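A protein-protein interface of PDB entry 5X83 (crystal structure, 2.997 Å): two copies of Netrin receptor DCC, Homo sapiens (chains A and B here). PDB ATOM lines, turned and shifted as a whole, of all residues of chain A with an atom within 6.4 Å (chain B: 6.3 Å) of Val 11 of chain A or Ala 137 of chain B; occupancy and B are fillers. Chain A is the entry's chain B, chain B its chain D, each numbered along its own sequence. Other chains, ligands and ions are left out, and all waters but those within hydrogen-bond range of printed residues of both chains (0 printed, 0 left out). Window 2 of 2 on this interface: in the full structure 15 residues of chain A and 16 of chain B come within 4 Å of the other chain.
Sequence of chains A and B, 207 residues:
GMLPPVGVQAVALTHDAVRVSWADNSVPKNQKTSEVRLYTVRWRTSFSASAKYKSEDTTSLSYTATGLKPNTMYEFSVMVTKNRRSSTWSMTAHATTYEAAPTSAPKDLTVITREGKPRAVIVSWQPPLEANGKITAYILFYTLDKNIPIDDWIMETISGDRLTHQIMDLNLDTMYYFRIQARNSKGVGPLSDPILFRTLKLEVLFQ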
ATOM      1  N   GLN A   9      -5.008  10.211   8.497  1.00  0.00           N
ATOM      2  CA  GLN A   9      -3.781  10.991   8.425  1.00  0.00           C
ATOM      3  C   GLN A   9      -2.606  10.121   7.997  1.00  0.00           C
ATOM      4  O   GLN A   9      -2.428   9.015   8.502  1.00  0.00           O
ATOM      5  CB  GLN A   9      -3.482  11.625   9.786  1.00  0.00           C
ATOM      6  CG  GLN A   9      -4.509  12.640  10.258  1.00  0.00           C
ATOM      7  CD  GLN A   9      -4.103  13.304  11.561  1.00  0.00           C
ATOM      8  OE1 GLN A   9      -3.014  13.060  12.080  1.00  0.00           O
ATOM      9  NE2 GLN A   9      -4.983  14.144  12.099  1.00  0.00           N
ATOM     10  N   ALA A  10      -1.805  10.621   7.062  1.00  0.00           N
ATOM     11  CA  ALA A  10      -0.631   9.888   6.603  1.00  0.00           C
ATOM     12  C   ALA A  10       0.636  10.699   6.843  1.00  0.00           C
ATOM     13  O   ALA A  10       0.795  11.788   6.289  1.00  0.00           O
ATOM     14  CB  ALA A  10      -0.764   9.525   5.133  1.00  0.00           C
ATOM     15  N   VAL A  11       1.535  10.173   7.667  1.00  0.00           N
ATOM     16  CA  VAL A  11       2.770  10.879   7.999  1.00  0.00           C
ATOM     17  C   VAL A  11       4.005  10.097   7.568  1.00  0.00           C
ATOM     18  O   VAL A  11       4.199   8.952   7.974  1.00  0.00           O
ATOM     19  CB  VAL A  11       2.872  11.169   9.512  1.00  0.00           C
ATOM     20  CG1 VAL A  11       4.169  11.898   9.825  1.00  0.00           C
ATOM     21  CG2 VAL A  11       1.672  11.975   9.987  1.00  0.00           C
ATOM     22  N   ALA A  12       4.841  10.724   6.749  1.00  0.00           N
ATOM     23  CA  ALA A  12       6.066  10.090   6.283  1.00  0.00           C
ATOM     24  C   ALA A  12       7.068   9.945   7.425  1.00  0.00           C
ATOM     25  O   ALA A  12       7.381  10.917   8.113  1.00  0.00           O
ATOM     26  CB  ALA A  12       6.673  10.886   5.139  1.00  0.00           C
ATOM     27  N   LEU A  13       7.574   8.730   7.620  1.00  0.00           N
ATOM     28  CA  LEU A  13       8.588   8.489   8.639  1.00  0.00           C
ATOM     29  C   LEU A  13       9.990   8.629   8.059  1.00  0.00           C
ATOM     30  O   LEU A  13      10.571   9.714   8.066  1.00  0.00           O
ATOM     31  CB  LEU A  13       8.411   7.102   9.257  1.00  0.00           C
ATOM     32  CG  LEU A  13       7.028   6.835   9.850  1.00  0.00           C
ATOM     33  CD1 LEU A  13       6.929   5.413  10.384  1.00  0.00           C
ATOM     34  CD2 LEU A  13       6.711   7.855  10.932  1.00  0.00           C
ATOM     35  N   ALA A  17       9.257   4.677   4.509  1.00  0.00           N
ATOM     36  CA  ALA A  17       8.153   4.335   5.402  1.00  0.00           C
ATOM     37  C   ALA A  17       7.171   5.487   5.602  1.00  0.00           C
ATOM     38  O   ALA A  17       7.570   6.645   5.744  1.00  0.00           O
ATOM     39  CB  ALA A  17       8.693   3.874   6.747  1.00  0.00           C
ATOM     40  N   VAL A  18       5.882   5.162   5.592  1.00  0.00           N
ATOM     41  CA  VAL A  18       4.836   6.130   5.905  1.00  0.00           C
ATOM     42  C   VAL A  18       3.814   5.485   6.841  1.00  0.00           C
ATOM     43  O   VAL A  18       3.407   4.344   6.629  1.00  0.00           O
ATOM     44  CB  VAL A  18       4.122   6.646   4.638  1.00  0.00           C
ATOM     45  CG1 VAL A  18       2.979   7.577   5.014  1.00  0.00           C
ATOM     46  CG2 VAL A  18       5.101   7.362   3.725  1.00  0.00           C
ATOM     47  N   ARG A  19       3.410   6.209   7.881  1.00  0.00           N
ATOM     48  CA  ARG A  19       2.469   5.666   8.856  1.00  0.00           C
ATOM     49  C   ARG A  19       1.078   6.282   8.726  1.00  0.00           C
ATOM     50  O   ARG A  19       0.864   7.444   9.074  1.00  0.00           O
ATOM     51  CB  ARG A  19       2.989   5.878  10.277  1.00  0.00           C
ATOM     52  CG  ARG A  19       2.144   5.187  11.333  1.00  0.00           C
ATOM     53  CD  ARG A  19       2.756   5.317  12.711  1.00  0.00           C
ATOM     54  NE  ARG A  19       4.122   4.812  12.754  1.00  0.00           N
ATOM     55  CZ  ARG A  19       4.435   3.532  12.905  1.00  0.00           C
ATOM     56  NH1 ARG A  19       5.707   3.157  12.932  1.00  0.00           N
ATOM     57  NH2 ARG A  19       3.475   2.622  13.023  1.00  0.00           N
ATOM     58  N   VAL A  20       0.137   5.492   8.224  1.00  0.00           N
ATOM     59  CA  VAL A  20      -1.254   5.912   8.134  1.00  0.00           C
ATOM     60  C   VAL A  20      -1.957   5.768   9.484  1.00  0.00           C
ATOM     61  O   VAL A  20      -1.685   4.830  10.234  1.00  0.00           O
ATOM     62  CB  VAL A  20      -2.008   5.094   7.071  1.00  0.00           C
ATOM     63  CG1 VAL A  20      -3.336   5.753   6.736  1.00  0.00           C
ATOM     64  CG2 VAL A  20      -1.164   4.968   5.820  1.00  0.00           C
ATOM     65  N   SER A  21      -2.851   6.702   9.797  1.00  0.00           N
ATOM     66  CA  SER A  21      -3.602   6.657  11.048  1.00  0.00           C
ATOM     67  C   SER A  21      -4.982   7.289  10.883  1.00  0.00           C
ATOM     68  O   SER A  21      -5.105   8.431  10.442  1.00  0.00           O
ATOM     69  CB  SER A  21      -2.829   7.359  12.165  1.00  0.00           C
ATOM     70  OG  SER A  21      -2.342   8.618  11.737  1.00  0.00           O
ATOM     71  N   PHE A  76      -2.994   7.743   0.127  1.00  0.00           N
ATOM     72  CA  PHE A  76      -3.469   6.658   0.982  1.00  0.00           C
ATOM     73  C   PHE A  76      -4.974   6.733   1.218  1.00  0.00           C
ATOM     74  O   PHE A  76      -5.529   7.818   1.380  1.00  0.00           O
ATOM     75  CB  PHE A  76      -2.737   6.683   2.326  1.00  0.00           C
ATOM     76  CG  PHE A  76      -1.243   6.607   2.208  1.00  0.00           C
ATOM     77  CD1 PHE A  76      -0.490   7.748   1.989  1.00  0.00           C
ATOM     78  CD2 PHE A  76      -0.590   5.395   2.327  1.00  0.00           C
ATOM     79  CE1 PHE A  76       0.886   7.678   1.883  1.00  0.00           C
ATOM     80  CE2 PHE A  76       0.785   5.318   2.221  1.00  0.00           C
ATOM     81  CZ  PHE A  76       1.523   6.461   1.997  1.00  0.00           C
ATOM     82  N   HIS A  94      -2.460  12.547   1.464  1.00  0.00           N
ATOM     83  CA  HIS A  94      -1.223  12.540   0.691  1.00  0.00           C
ATOM     84  C   HIS A  94       0.014  12.713   1.563  1.00  0.00           C
ATOM     85  O   HIS A  94       0.038  13.547   2.468  1.00  0.00           O
ATOM     86  CB  HIS A  94      -1.257  13.634  -0.373  1.00  0.00           C
ATOM     87  CG  HIS A  94      -2.332  13.447  -1.397  1.00  0.00           C
ATOM     88  ND1 HIS A  94      -2.235  12.530  -2.419  1.00  0.00           N
ATOM     89  CD2 HIS A  94      -3.527  14.065  -1.558  1.00  0.00           C
ATOM     90  CE1 HIS A  94      -3.324  12.587  -3.166  1.00  0.00           C
ATOM     91  NE2 HIS A  94      -4.124  13.511  -2.664  1.00  0.00           N
ATOM     92  N   ALA A  95       1.042  11.922   1.279  1.00  0.00           N
ATOM     93  CA  ALA A  95       2.296  12.005   2.016  1.00  0.00           C
ATOM     94  C   ALA A  95       3.482  11.781   1.088  1.00  0.00           C
ATOM     95  O   ALA A  95       3.478  10.857   0.274  1.00  0.00           O
ATOM     96  CB  ALA A  95       2.312  10.999   3.152  1.00  0.00           C
ATOM     97  N   LYS B 134      14.536  18.366  11.466  1.00  0.00           N
ATOM     98  CA  LYS B 134      13.103  18.636  11.455  1.00  0.00           C
ATOM     99  C   LYS B 134      12.328  17.425  11.951  1.00  0.00           C
ATOM    100  O   LYS B 134      12.444  16.335  11.390  1.00  0.00           O
ATOM    101  CB  LYS B 134      12.623  19.017  10.055  1.00  0.00           C
ATOM    102  CG  LYS B 134      11.121  19.243   9.974  1.00  0.00           C
ATOM    103  CD  LYS B 134      10.674  19.579   8.564  1.00  0.00           C
ATOM    104  CE  LYS B 134       9.163  19.482   8.429  1.00  0.00           C
ATOM    105  NZ  LYS B 134       8.676  20.102   7.164  1.00  0.00           N
ATOM    106  N   ILE B 135      11.538  17.623  13.002  1.00  0.00           N
ATOM    107  CA  ILE B 135      10.781  16.532  13.600  1.00  0.00           C
ATOM    108  C   ILE B 135       9.668  16.093  12.658  1.00  0.00           C
ATOM    109  O   ILE B 135       8.772  16.872  12.333  1.00  0.00           O
ATOM    110  CB  ILE B 135      10.177  16.940  14.956  1.00  0.00           C
ATOM    111  CG1 ILE B 135      11.283  17.340  15.932  1.00  0.00           C
ATOM    112  CG2 ILE B 135       9.355  15.801  15.535  1.00  0.00           C
ATOM    113  CD1 ILE B 135      12.292  16.242  16.181  1.00  0.00           C
ATOM    114  N   THR B 136       9.735  14.843  12.213  1.00  0.00           N
ATOM    115  CA  THR B 136       8.767  14.328  11.254  1.00  0.00           C
ATOM    116  C   THR B 136       7.489  13.887  11.952  1.00  0.00           C
ATOM    117  O   THR B 136       6.384  14.148  11.473  1.00  0.00           O
ATOM    118  CB  THR B 136       9.334  13.140  10.456  1.00  0.00           C
ATOM    119  OG1 THR B 136       9.655  12.066  11.350  1.00  0.00           O
ATOM    120  CG2 THR B 136      10.584  13.553   9.698  1.00  0.00           C
ATOM    121  N   ALA B 137       7.646  13.226  13.092  1.00  0.00           N
ATOM    122  CA  ALA B 137       6.505  12.700  13.827  1.00  0.00           C
ATOM    123  C   ALA B 137       6.801  12.561  15.315  1.00  0.00           C
ATOM    124  O   ALA B 137       7.952  12.409  15.720  1.00  0.00           O
ATOM    125  CB  ALA B 137       6.085  11.357  13.249  1.00  0.00           C
ATOM    126  N   TYR B 138       5.753  12.628  16.125  1.00  0.00           N
ATOM    127  CA  TYR B 138       5.857  12.313  17.543  1.00  0.00           C
ATOM    128  C   TYR B 138       5.212  10.964  17.828  1.00  0.00           C
ATOM    129  O   TYR B 138       4.204  10.612  17.219  1.00  0.00           O
ATOM    130  CB  TYR B 138       5.205  13.402  18.395  1.00  0.00           C
ATOM    131  CG  TYR B 138       5.970  14.705  18.420  1.00  0.00           C
ATOM    132  CD1 TYR B 138       6.989  14.915  19.340  1.00  0.00           C
ATOM    133  CD2 TYR B 138       5.678  15.721  17.522  1.00  0.00           C
ATOM    134  CE1 TYR B 138       7.692  16.105  19.367  1.00  0.00           C
ATOM    135  CE2 TYR B 138       6.376  16.913  17.541  1.00  0.00           C
ATOM    136  CZ  TYR B 138       7.380  17.099  18.465  1.00  0.00           C
ATOM    137  OH  TYR B 138       8.075  18.285  18.483  1.00  0.00           O
ATOM    138  N   ILE B 139       5.813  10.199  18.732  1.00  0.00           N
ATOM    139  CA  ILE B 139       5.245   8.923  19.146  1.00  0.00           C
ATOM    140  C   ILE B 139       4.855   8.976  20.619  1.00  0.00           C
ATOM    141  O   ILE B 139       5.703   9.188  21.485  1.00  0.00           O
ATOM    142  CB  ILE B 139       6.224   7.762  18.914  1.00  0.00           C
ATOM    143  CG1 ILE B 139       6.779   7.799  17.488  1.00  0.00           C
ATOM    144  CG2 ILE B 139       5.537   6.435  19.175  1.00  0.00           C
ATOM    145  CD1 ILE B 139       5.728   7.604  16.422  1.00  0.00           C
ATOM    146  N   THR B 157       0.578   8.005  17.024  1.00  0.00           N
ATOM    147  CA  THR B 157       1.551   8.763  16.250  1.00  0.00           C
ATOM    148  C   THR B 157       0.970  10.093  15.795  1.00  0.00           C
ATOM    149  O   THR B 157       0.029  10.137  15.004  1.00  0.00           O
ATOM    150  CB  THR B 157       2.043   7.971  15.030  1.00  0.00           C
ATOM    151  OG1 THR B 157       2.694   6.774  15.474  1.00  0.00           O
ATOM    152  CG2 THR B 157       3.027   8.799  14.223  1.00  0.00           C
ATOM    153  N   ILE B 158       1.538  11.176  16.315  1.00  0.00           N
ATOM    154  CA  ILE B 158       1.090  12.522  15.990  1.00  0.00           C
ATOM    155  C   ILE B 158       2.093  13.197  15.057  1.00  0.00           C
ATOM    156  O   ILE B 158       3.296  12.960  15.156  1.00  0.00           O
ATOM    157  CB  ILE B 158       0.906  13.378  17.267  1.00  0.00           C
ATOM    158  CG1 ILE B 158       0.092  12.622  18.321  1.00  0.00           C
ATOM    159  CG2 ILE B 158       0.257  14.708  16.944  1.00  0.00           C
ATOM    160  CD1 ILE B 158       0.935  11.919  19.369  1.00  0.00           C
ATOM    161  N   SER B 159       1.596  14.028  14.146  1.00  0.00           N
ATOM    162  CA  SER B 159       2.454  14.750  13.216  1.00  0.00           C
ATOM    163  C   SER B 159       3.339  15.767  13.935  1.00  0.00           C
ATOM    164  O   SER B 159       2.988  16.267  15.005  1.00  0.00           O
ATOM    165  CB  SER B 159       1.611  15.450  12.147  1.00  0.00           C
ATOM    166  OG  SER B 159       2.385  16.393  11.422  1.00  0.00           O
ATOM    167  N   GLY B 160       4.490  16.061  13.338  1.00  0.00           N
ATOM    168  CA  GLY B 160       5.452  16.988  13.911  1.00  0.00           C
ATOM    169  C   GLY B 160       4.954  18.419  14.031  1.00  0.00           C
ATOM    170  O   GLY B 160       5.554  19.229  14.736  1.00  0.00           O
ATOM    171  N   GLN B 181       8.127  10.439  22.562  1.00  0.00           N
ATOM    172  CA  GLN B 181       9.415  10.569  21.891  1.00  0.00           C
ATOM    173  C   GLN B 181       9.260  11.251  20.536  1.00  0.00           C
ATOM    174  O   GLN B 181       8.179  11.240  19.947  1.00  0.00           O
ATOM    175  CB  GLN B 181      10.078   9.198  21.729  1.00  0.00           C
ATOM    176  CG  GLN B 181       9.351   8.241  20.794  1.00  0.00           C
ATOM    177  CD  GLN B 181      10.026   6.880  20.714  1.00  0.00           C
ATOM    178  OE1 GLN B 181      11.158   6.708  21.167  1.00  0.00           O
ATOM    179  NE2 GLN B 181       9.335   5.909  20.126  1.00  0.00           N
ATOM    180  N   ALA B 182      10.342  11.851  20.053  1.00  0.00           N
ATOM    181  CA  ALA B 182      10.330  12.565  18.779  1.00  0.00           C
ATOM    182  C   ALA B 182      11.032  11.757  17.693  1.00  0.00           C
ATOM    183  O   ALA B 182      12.089  11.173  17.930  1.00  0.00           O
ATOM    184  CB  ALA B 182      10.980  13.931  18.929  1.00  0.00           C
ATOM    185  N   ARG B 183      10.434  11.716  16.507  1.00  0.00           N
ATOM    186  CA  ARG B 183      11.050  11.057  15.362  1.00  0.00           C
ATOM    187  C   ARG B 183      11.675  12.103  14.437  1.00  0.00           C
ATOM    188  O   ARG B 183      11.539  13.307  14.661  1.00  0.00           O
ATOM    189  CB  ARG B 183      10.022  10.205  14.601  1.00  0.00           C
ATOM    190  CG  ARG B 183      10.626   9.160  13.665  1.00  0.00           C
ATOM    191  CD  ARG B 183       9.608   8.150  13.183  1.00  0.00           C
ATOM    192  NE  ARG B 183      10.209   7.182  12.270  1.00  0.00           N
ATOM    193  CZ  ARG B 183      10.723   6.017  12.652  1.00  0.00           C
ATOM    194  NH1 ARG B 183      10.705   5.669  13.932  1.00  0.00           N
ATOM    195  NH2 ARG B 183      11.251   5.197  11.754  1.00  0.00           N
ATOM    196  N   ASN B 184      12.352  11.630  13.397  1.00  0.00           N
ATOM    197  CA  ASN B 184      13.162  12.465  12.528  1.00  0.00           C
ATOM    198  C   ASN B 184      13.508  11.659  11.278  1.00  0.00           C
ATOM    199  O   ASN B 184      13.461  10.428  11.308  1.00  0.00           O
ATOM    200  CB  ASN B 184      14.418  12.934  13.270  1.00  0.00           C
ATOM    201  CG  ASN B 184      15.436  13.570  12.358  1.00  0.00           C
ATOM    202  OD1 ASN B 184      16.415  12.936  11.965  1.00  0.00           O
ATOM    203  ND2 ASN B 184      15.211  14.832  12.012  1.00  0.00           N
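Val 11 of chain A touches Thr 136 of chain B. Val 11 of chain A touches Ala 137 of chain B. Thr 136 of chain B touches Ala 12 of chain A. Leu 13 of chain A touches Arg 183 of chain B. Thr 157 of chain B touches Arg 19 of chain A.
Of the 13 printed residues of chain A, 4 touch a printed residue of chain B. Printed residues of chain A that touch a printed residue of chain B: Val 11, Ala 12, Leu 13 and Arg 19. Hydrophobic or aromatic side chains of chain A that line the printed part of chain B: Val 11 and Leu 13. Hydrophobic or aromatic side chains of chain B that line the printed part of chain A: Ala 137. Among the printed residues, no Asp or Glu carboxylate lies within 4 Å of a Lys or Arg side-chain nitrogen of the other chain.
No position is printed for both chains.
N of Arg 19 of chain A is in hydrogen-bond range of O of Val 11 of chain A (2.9 Å). OG1 of Thr 136 of chain B lies within hydrogen-bond range of N of Asn 184 of chain B, 3.4 Å away. The backbone carbonyl oxygen (O) of Arg 183 of chain B sits at hydrogen-bond distance from the backbone NH (N) of Thr 136 of chain B, at 3.4 Å. O of Thr 136 of chain B is in hydrogen-bond range of N of Gly 160 of chain B (3.3 Å). The backbone NH (N) of Arg 183 of chain B sits at hydrogen-bond distance from the backbone carbonyl oxygen (O) of Ala 137 of chain B, 2.7 Å away.
Printed residues of chain B within 4 Å of Val 11 of chain A: Thr 136 (3.6 Å) and Ala 137 (3.96 Å). Of chain A, only Val 11 comes within 4 Å of Ala 137 of chain B. Printed residues of chain B within 4 Å of Arg 19 of chain A: Thr 157. Of the printed residues of chain A, Thr 136 of chain B touches Val 11 and Ala 12. The nearest residue of chain B that does not touch Val 11 of chain A is Ser 159 of chain B (4.1 Å). The nearest printed residue of chain B that does not touch Ala 12 of chain A is Ala 137 of chain B (5.3 Å).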
